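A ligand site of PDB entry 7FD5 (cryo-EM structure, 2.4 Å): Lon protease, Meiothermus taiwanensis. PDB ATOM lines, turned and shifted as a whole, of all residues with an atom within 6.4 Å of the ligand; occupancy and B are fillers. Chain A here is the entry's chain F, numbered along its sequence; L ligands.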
ATOM      1  N   ASP A 318     -10.638   9.040  -0.272  1.00  0.00           N
ATOM      2  CA  ASP A 318      -9.682   9.525  -1.255  1.00  0.00           C
ATOM      3  C   ASP A 318     -10.313  10.048  -2.531  1.00  0.00           C
ATOM      4  O   ASP A 318      -9.578  10.470  -3.428  1.00  0.00           O
ATOM      5  CB  ASP A 318      -8.672   8.430  -1.612  1.00  0.00           C
ATOM      6  CG  ASP A 318      -7.616   8.228  -0.537  1.00  0.00           C
ATOM      7  OD1 ASP A 318      -7.292   9.214   0.160  1.00  0.00           O
ATOM      8  OD2 ASP A 318      -7.099   7.104  -0.398  1.00  0.00           O
ATOM      9  N   HIS A 319     -11.637  10.035  -2.652  1.00  0.00           N
ATOM     10  CA  HIS A 319     -12.314  10.562  -3.832  1.00  0.00           C
ATOM     11  C   HIS A 319     -13.629  11.189  -3.433  1.00  0.00           C
ATOM     12  O   HIS A 319     -14.047  11.139  -2.281  1.00  0.00           O
ATOM     13  CB  HIS A 319     -12.584   9.484  -4.864  1.00  0.00           C
ATOM     14  CG  HIS A 319     -11.352   8.903  -5.452  1.00  0.00           C
ATOM     15  ND1 HIS A 319     -10.582   9.577  -6.373  1.00  0.00           N
ATOM     16  CD2 HIS A 319     -10.716   7.730  -5.222  1.00  0.00           C
ATOM     17  CE1 HIS A 319      -9.539   8.838  -6.692  1.00  0.00           C
ATOM     18  NE2 HIS A 319      -9.599   7.710  -6.012  1.00  0.00           N
ATOM     19  N   TYR A 320     -14.263  11.796  -4.412  1.00  0.00           N
ATOM     20  CA  TYR A 320     -15.605  12.329  -4.281  1.00  0.00           C
ATOM     21  C   TYR A 320     -16.509  11.606  -5.259  1.00  0.00           C
ATOM     22  O   TYR A 320     -16.107  11.337  -6.391  1.00  0.00           O
ATOM     23  CB  TYR A 320     -15.646  13.826  -4.571  1.00  0.00           C
ATOM     24  CG  TYR A 320     -17.004  14.426  -4.369  1.00  0.00           C
ATOM     25  CD1 TYR A 320     -17.426  14.790  -3.111  1.00  0.00           C
ATOM     26  CD2 TYR A 320     -17.866  14.619  -5.436  1.00  0.00           C
ATOM     27  CE1 TYR A 320     -18.668  15.352  -2.922  1.00  0.00           C
ATOM     28  CE2 TYR A 320     -19.107  15.169  -5.253  1.00  0.00           C
ATOM     29  CZ  TYR A 320     -19.507  15.529  -3.999  1.00  0.00           C
ATOM     30  OH  TYR A 320     -20.743  16.072  -3.834  1.00  0.00           O
ATOM     31  N   GLY A 321     -17.730  11.328  -4.816  1.00  0.00           N
ATOM     32  CA  GLY A 321     -18.729  10.784  -5.728  1.00  0.00           C
ATOM     33  C   GLY A 321     -18.364   9.393  -6.187  1.00  0.00           C
ATOM     34  O   GLY A 321     -17.778   8.602  -5.439  1.00  0.00           O
ATOM     35  N   LEU A 322     -18.703   9.116  -7.449  1.00  0.00           N
ATOM     36  CA  LEU A 322     -18.325   7.893  -8.170  1.00  0.00           C
ATOM     37  C   LEU A 322     -18.792   6.622  -7.455  1.00  0.00           C
ATOM     38  O   LEU A 322     -18.003   5.745  -7.138  1.00  0.00           O
ATOM     39  CB  LEU A 322     -16.816   7.855  -8.409  1.00  0.00           C
ATOM     40  CG  LEU A 322     -16.203   8.819  -9.405  1.00  0.00           C
ATOM     41  CD1 LEU A 322     -14.704   8.618  -9.426  1.00  0.00           C
ATOM     42  CD2 LEU A 322     -16.795   8.559 -10.769  1.00  0.00           C
ATOM     43  N   GLY A 355     -12.137   5.060 -19.764  1.00  0.00           N
ATOM     44  CA  GLY A 355     -12.764   6.357 -19.696  1.00  0.00           C
ATOM     45  C   GLY A 355     -11.905   7.420 -20.360  1.00  0.00           C
ATOM     46  O   GLY A 355     -10.793   7.138 -20.809  1.00  0.00           O
ATOM     47  N   PRO A 356     -12.398   8.650 -20.420  1.00  0.00           N
ATOM     48  CA  PRO A 356     -11.644   9.728 -21.072  1.00  0.00           C
ATOM     49  C   PRO A 356     -10.431  10.136 -20.245  1.00  0.00           C
ATOM     50  O   PRO A 356     -10.256   9.650 -19.119  1.00  0.00           O
ATOM     51  CB  PRO A 356     -12.673  10.868 -21.149  1.00  0.00           C
ATOM     52  CG  PRO A 356     -13.593  10.608 -20.040  1.00  0.00           C
ATOM     53  CD  PRO A 356     -13.701   9.115 -19.930  1.00  0.00           C
ATOM     54  N   PRO A 357      -9.556  10.992 -20.757  1.00  0.00           N
ATOM     55  CA  PRO A 357      -8.536  11.585 -19.880  1.00  0.00           C
ATOM     56  C   PRO A 357      -9.159  12.615 -18.957  1.00  0.00           C
ATOM     57  O   PRO A 357     -10.175  13.236 -19.265  1.00  0.00           O
ATOM     58  CB  PRO A 357      -7.563  12.247 -20.865  1.00  0.00           C
ATOM     59  CG  PRO A 357      -7.799  11.553 -22.141  1.00  0.00           C
ATOM     60  CD  PRO A 357      -9.248  11.233 -22.177  1.00  0.00           C
ATOM     61  N   GLY A 358      -8.536  12.783 -17.804  1.00  0.00           N
ATOM     62  CA  GLY A 358      -8.973  13.772 -16.842  1.00  0.00           C
ATOM     63  C   GLY A 358      -9.857  13.217 -15.752  1.00  0.00           C
ATOM     64  O   GLY A 358     -10.003  13.868 -14.719  1.00  0.00           O
ATOM     65  N   VAL A 359     -10.460  12.060 -15.959  1.00  0.00           N
ATOM     66  CA  VAL A 359     -11.140  11.398 -14.867  1.00  0.00           C
ATOM     67  C   VAL A 359     -10.107  10.745 -13.957  1.00  0.00           C
ATOM     68  O   VAL A 359      -8.960  10.503 -14.335  1.00  0.00           O
ATOM     69  CB  VAL A 359     -12.151  10.366 -15.394  1.00  0.00           C
ATOM     70  CG1 VAL A 359     -13.124  11.011 -16.341  1.00  0.00           C
ATOM     71  CG2 VAL A 359     -11.449   9.221 -16.083  1.00  0.00           C
ATOM     72  N   GLY A 360     -10.511  10.475 -12.725  1.00  0.00           N
ATOM     73  CA  GLY A 360      -9.555   9.925 -11.783  1.00  0.00           C
ATOM     74  C   GLY A 360      -9.382   8.437 -11.953  1.00  0.00           C
ATOM     75  O   GLY A 360     -10.258   7.661 -11.588  1.00  0.00           O
ATOM     76  N   LYS A 361      -8.262   8.020 -12.527  1.00  0.00           N
ATOM     77  CA  LYS A 361      -8.031   6.593 -12.715  1.00  0.00           C
ATOM     78  C   LYS A 361      -6.835   6.091 -11.935  1.00  0.00           C
ATOM     79  O   LYS A 361      -6.977   5.142 -11.153  1.00  0.00           O
ATOM     80  CB  LYS A 361      -7.879   6.283 -14.200  1.00  0.00           C
ATOM     81  CG  LYS A 361      -9.158   6.447 -14.981  1.00  0.00           C
ATOM     82  CD  LYS A 361      -9.023   5.922 -16.386  1.00  0.00           C
ATOM     83  CE  LYS A 361      -8.220   6.854 -17.247  1.00  0.00           C
ATOM     84  NZ  LYS A 361      -8.177   6.382 -18.650  1.00  0.00           N
ATOM     85  N   THR A 362      -5.660   6.688 -12.119  1.00  0.00           N
ATOM     86  CA  THR A 362      -4.488   6.278 -11.356  1.00  0.00           C
ATOM     87  C   THR A 362      -4.624   6.645  -9.886  1.00  0.00           C
ATOM     88  O   THR A 362      -4.033   5.974  -9.026  1.00  0.00           O
ATOM     89  CB  THR A 362      -3.241   6.901 -11.933  1.00  0.00           C
ATOM     90  OG1 THR A 362      -3.329   8.321 -11.816  1.00  0.00           O
ATOM     91  CG2 THR A 362      -3.117   6.560 -13.394  1.00  0.00           C
ATOM     92  N   SER A 363      -5.402   7.683  -9.592  1.00  0.00           N
ATOM     93  CA  SER A 363      -5.752   7.990  -8.220  1.00  0.00           C
ATOM     94  C   SER A 363      -6.584   6.883  -7.589  1.00  0.00           C
ATOM     95  O   SER A 363      -6.432   6.612  -6.391  1.00  0.00           O
ATOM     96  CB  SER A 363      -6.476   9.322  -8.178  1.00  0.00           C
ATOM     97  OG  SER A 363      -7.617   9.266  -9.001  1.00  0.00           O
ATOM     98  N   ARG A 378       3.215   2.191 -10.462  1.00  0.00           N
ATOM     99  CA  ARG A 378       2.683   2.275 -11.854  1.00  0.00           C
ATOM    100  C   ARG A 378       3.743   1.862 -12.870  1.00  0.00           C
ATOM    101  O   ARG A 378       4.835   2.467 -12.859  1.00  0.00           O
ATOM    102  CB  ARG A 378       2.255   3.722 -12.137  1.00  0.00           C
ATOM    103  CG  ARG A 378       0.827   3.879 -12.626  1.00  0.00           C
ATOM    104  CD  ARG A 378       0.419   5.338 -12.669  1.00  0.00           C
ATOM    105  NE  ARG A 378       1.277   6.107 -13.557  1.00  0.00           N
ATOM    106  CZ  ARG A 378       1.164   7.419 -13.757  1.00  0.00           C
ATOM    107  NH1 ARG A 378       0.243   8.108 -13.118  1.00  0.00           N
ATOM    108  NH2 ARG A 378       1.989   8.034 -14.579  1.00  0.00           N
ATOM    109  N   THR A 470      -5.498   0.326 -16.705  1.00  0.00           N
ATOM    110  CA  THR A 470      -6.280   1.388 -17.302  1.00  0.00           C
ATOM    111  C   THR A 470      -6.001   1.441 -18.795  1.00  0.00           C
ATOM    112  O   THR A 470      -4.858   1.288 -19.227  1.00  0.00           O
ATOM    113  CB  THR A 470      -5.974   2.752 -16.686  1.00  0.00           C
ATOM    114  OG1 THR A 470      -4.585   3.045 -16.819  1.00  0.00           O
ATOM    115  CG2 THR A 470      -6.378   2.788 -15.223  1.00  0.00           C
ATOM    116  N   TYR A 493     -17.826  13.735 -15.552  1.00  0.00           N
ATOM    117  CA  TYR A 493     -18.353  14.394 -14.368  1.00  0.00           C
ATOM    118  C   TYR A 493     -19.424  15.403 -14.736  1.00  0.00           C
ATOM    119  O   TYR A 493     -19.644  15.710 -15.910  1.00  0.00           O
ATOM    120  CB  TYR A 493     -17.234  15.051 -13.586  1.00  0.00           C
ATOM    121  CG  TYR A 493     -16.200  14.056 -13.155  1.00  0.00           C
ATOM    122  CD1 TYR A 493     -16.385  13.283 -12.031  1.00  0.00           C
ATOM    123  CD2 TYR A 493     -15.042  13.869 -13.887  1.00  0.00           C
ATOM    124  CE1 TYR A 493     -15.450  12.357 -11.649  1.00  0.00           C
ATOM    125  CE2 TYR A 493     -14.114  12.962 -13.513  1.00  0.00           C
ATOM    126  CZ  TYR A 493     -14.316  12.210 -12.400  1.00  0.00           C
ATOM    127  OH  TYR A 493     -13.373  11.296 -12.043  1.00  0.00           O
ATOM    128  N   ILE A 501     -15.094  18.666  -6.479  1.00  0.00           N
ATOM    129  CA  ILE A 501     -13.706  18.251  -6.617  1.00  0.00           C
ATOM    130  C   ILE A 501     -12.774  19.450  -6.592  1.00  0.00           C
ATOM    131  O   ILE A 501     -11.723  19.405  -5.953  1.00  0.00           O
ATOM    132  CB  ILE A 501     -13.523  17.413  -7.891  1.00  0.00           C
ATOM    133  CG1 ILE A 501     -14.301  16.117  -7.801  1.00  0.00           C
ATOM    134  CG2 ILE A 501     -12.072  17.041  -8.104  1.00  0.00           C
ATOM    135  CD1 ILE A 501     -14.442  15.407  -9.124  1.00  0.00           C
ATOM    136  N   TYR A 505     -10.195  19.190  -3.483  1.00  0.00           N
ATOM    137  CA  TYR A 505      -8.907  18.611  -3.774  1.00  0.00           C
ATOM    138  C   TYR A 505      -8.031  19.399  -4.730  1.00  0.00           C
ATOM    139  O   TYR A 505      -6.833  19.113  -4.797  1.00  0.00           O
ATOM    140  CB  TYR A 505      -9.074  17.205  -4.373  1.00  0.00           C
ATOM    141  CG  TYR A 505      -9.660  16.152  -3.448  1.00  0.00           C
ATOM    142  CD1 TYR A 505      -9.686  16.329  -2.069  1.00  0.00           C
ATOM    143  CD2 TYR A 505     -10.175  14.984  -3.956  1.00  0.00           C
ATOM    144  CE1 TYR A 505     -10.223  15.366  -1.240  1.00  0.00           C
ATOM    145  CE2 TYR A 505     -10.708  14.015  -3.145  1.00  0.00           C
ATOM    146  CZ  TYR A 505     -10.726  14.205  -1.791  1.00  0.00           C
ATOM    147  OH  TYR A 505     -11.266  13.220  -0.998  1.00  0.00           O
ATOM    148  N   LEU A 506      -8.568  20.362  -5.481  1.00  0.00           N
ATOM    149  CA  LEU A 506      -7.784  21.002  -6.539  1.00  0.00           C
ATOM    150  C   LEU A 506      -7.314  22.400  -6.188  1.00  0.00           C
ATOM    151  O   LEU A 506      -6.135  22.707  -6.389  1.00  0.00           O
ATOM    152  CB  LEU A 506      -8.580  21.052  -7.834  1.00  0.00           C
ATOM    153  CG  LEU A 506      -8.872  19.704  -8.463  1.00  0.00           C
ATOM    154  CD1 LEU A 506      -9.691  19.925  -9.691  1.00  0.00           C
ATOM    155  CD2 LEU A 506      -7.606  18.974  -8.805  1.00  0.00           C
ATOM    156  N   LYS A 509      -4.362  22.418  -3.364  1.00  0.00           N
ATOM    157  CA  LYS A 509      -3.071  21.989  -3.881  1.00  0.00           C
ATOM    158  C   LYS A 509      -2.420  23.068  -4.733  1.00  0.00           C
ATOM    159  O   LYS A 509      -1.238  23.392  -4.548  1.00  0.00           O
ATOM    160  CB  LYS A 509      -3.251  20.718  -4.692  1.00  0.00           C
ATOM    161  CG  LYS A 509      -1.989  20.230  -5.305  1.00  0.00           C
ATOM    162  CD  LYS A 509      -2.255  19.005  -6.133  1.00  0.00           C
ATOM    163  CE  LYS A 509      -0.967  18.456  -6.696  1.00  0.00           C
ATOM    164  NZ  LYS A 509      -0.354  19.401  -7.653  1.00  0.00           N
ATOM    165  N   VAL A 540     -10.998  16.910 -15.839  1.00  0.00           N
ATOM    166  CA  VAL A 540     -10.863  18.021 -14.917  1.00  0.00           C
ATOM    167  C   VAL A 540      -9.504  18.708 -15.086  1.00  0.00           C
ATOM    168  O   VAL A 540      -9.160  19.621 -14.315  1.00  0.00           O
ATOM    169  CB  VAL A 540     -11.122  17.515 -13.480  1.00  0.00           C
ATOM    170  CG1 VAL A 540      -9.936  16.774 -12.925  1.00  0.00           C
ATOM    171  CG2 VAL A 540     -11.658  18.606 -12.567  1.00  0.00           C
ATOM    172  N   ARG A 541      -8.733  18.307 -16.102  1.00  0.00           N
ATOM    173  CA  ARG A 541      -7.387  18.865 -16.316  1.00  0.00           C
ATOM    174  C   ARG A 541      -7.428  20.358 -16.648  1.00  0.00           C
ATOM    175  O   ARG A 541      -6.565  21.127 -16.175  1.00  0.00           O
ATOM    176  CB  ARG A 541      -6.682  18.122 -17.437  1.00  0.00           C
ATOM    177  CG  ARG A 541      -6.391  16.703 -17.144  1.00  0.00           C
ATOM    178  CD  ARG A 541      -5.661  16.070 -18.307  1.00  0.00           C
ATOM    179  NE  ARG A 541      -5.491  14.637 -18.105  1.00  0.00           N
ATOM    180  CZ  ARG A 541      -4.460  14.080 -17.490  1.00  0.00           C
ATOM    181  NH1 ARG A 541      -3.478  14.829 -17.002  1.00  0.00           N
ATOM    182  NH2 ARG A 541      -4.400  12.762 -17.366  1.00  0.00           N
ATOM    183  N   GLU A 544      -7.783  22.428 -13.582  1.00  0.00           N
ATOM    184  CA  GLU A 544      -6.499  22.537 -12.905  1.00  0.00           C
ATOM    185  C   GLU A 544      -5.636  23.621 -13.499  1.00  0.00           C
ATOM    186  O   GLU A 544      -5.005  24.402 -12.773  1.00  0.00           O
ATOM    187  CB  GLU A 544      -5.752  21.221 -12.957  1.00  0.00           C
ATOM    188  CG  GLU A 544      -6.341  20.143 -12.145  1.00  0.00           C
ATOM    189  CD  GLU A 544      -5.573  18.864 -12.270  1.00  0.00           C
ATOM    190  OE1 GLU A 544      -4.643  18.799 -13.101  1.00  0.00           O
ATOM    191  OE2 GLU A 544      -5.898  17.908 -11.542  1.00  0.00           O
HETATM  192  P1  LIG L   1      -6.305  10.229 -16.129  1.00  0.00           P
HETATM  193  O1  LIG L   1      -7.588  10.319 -16.907  1.00  0.00           O
HETATM  194  O2  LIG L   1      -5.057  10.378 -16.966  1.00  0.00           O
HETATM  195  O3  LIG L   1      -6.276   9.134 -15.112  1.00  0.00           O
HETATM  196  P2  LIG L   1      -5.600  11.603 -13.840  1.00  0.00           P
HETATM  197  O4  LIG L   1      -6.438  10.883 -12.822  1.00  0.00           O
HETATM  198  O5  LIG L   1      -4.159  11.209 -14.059  1.00  0.00           O
HETATM  199  O6  LIG L   1      -6.349  11.570 -15.246  1.00  0.00           O
HETATM  200  O7  LIG L   1      -5.618  13.148 -13.466  1.00  0.00           O
HETATM  201  C1  LIG L   1      -6.827  13.730 -13.003  1.00  0.00           C
HETATM  202  C2  LIG L   1      -6.463  14.523 -11.772  1.00  0.00           C
HETATM  203  O8  LIG L   1      -7.639  14.903 -11.068  1.00  0.00           O
HETATM  204  C3  LIG L   1      -5.655  13.667 -10.816  1.00  0.00           C
HETATM  205  O9  LIG L   1      -4.334  14.193 -10.742  1.00  0.00           O
HETATM  206  C4  LIG L   1      -6.294  13.831  -9.467  1.00  0.00           C
HETATM  207  O10 LIG L   1      -5.317  14.303  -8.558  1.00  0.00           O
HETATM  208  C5  LIG L   1      -7.340  14.896  -9.685  1.00  0.00           C
HETATM  209  N1  LIG L   1      -8.516  14.573  -8.868  1.00  0.00           N
HETATM  210  C6  LIG L   1      -8.667  14.903  -7.585  1.00  0.00           C
HETATM  211  N2  LIG L   1      -9.851  14.475  -7.103  1.00  0.00           N
HETATM  212  C7  LIG L   1     -10.481  13.854  -8.090  1.00  0.00           C
HETATM  213  C8  LIG L   1     -11.772  13.170  -8.221  1.00  0.00           C
HETATM  214  N3  LIG L   1     -12.623  13.076  -7.195  1.00  0.00           N
HETATM  215  N4  LIG L   1     -12.053  12.653  -9.418  1.00  0.00           N
HETATM  216  C9  LIG L   1     -11.191  12.756 -10.445  1.00  0.00           C
HETATM  217  N5  LIG L   1     -10.006  13.352 -10.397  1.00  0.00           N
HETATM  218  C10 LIG L   1      -9.596  13.912  -9.248  1.00  0.00           C
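An oxygen (O1) of the ligand lies within hydrogen-bond range of the backbone NH of Gly 358 (2.8 Å).
The backbone NH of Lys 361 lies within hydrogen-bond range of an oxygen (O4) of the ligand, at 3.4 Å.
The backbone NH (N) of Val 359 lies within hydrogen-bond range of an oxygen (O1) of the ligand (3.5 Å).
An oxygen (O1) of the ligand lies close to the backbone carbonyl oxygen of Val 359, at 2.9 Å.
OH of Tyr 493 lies close to N4 of the ligand (3.2 Å).
An oxygen (O2) of the ligand lies within salt-bridge range of the guanidinium group of Arg 541, at 2.5 Å.
The backbone carbonyl oxygen (O) of Ile 501 lies within hydrogen-bond range of the backbone NH (N) of Leu 506, at 3.3 Å.
NZ of Lys 361 sits at hydrogen-bond distance from O of Gly 355, 3.5 Å away.
The backbone carbonyl oxygen (O) of Gly 358 is in hydrogen-bond range of the backbone NH (N) of Val 540 (3.4 Å).
OH of Tyr 493 lies within hydrogen-bond range of N of Gly 360, at 3.1 Å.
The backbone NH (N) of Tyr 320 lies close to a nitrogen (N3) of the ligand (3.5 Å).
Pro 356 touches the ligand (O to O1, 3.5 Å).
Pro 357 touches the ligand.
N of Gly 360 touches C9 of the ligand (3.3 Å).
Thr 362 touches the ligand.
Ile 501 touches the ligand.
Tyr 505 touches the ligand.
Val 540 touches the ligand.
Glu 544 touches the ligand.
The nearest printed residue that does not touch the ligand is His 319 (4.1 Å).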
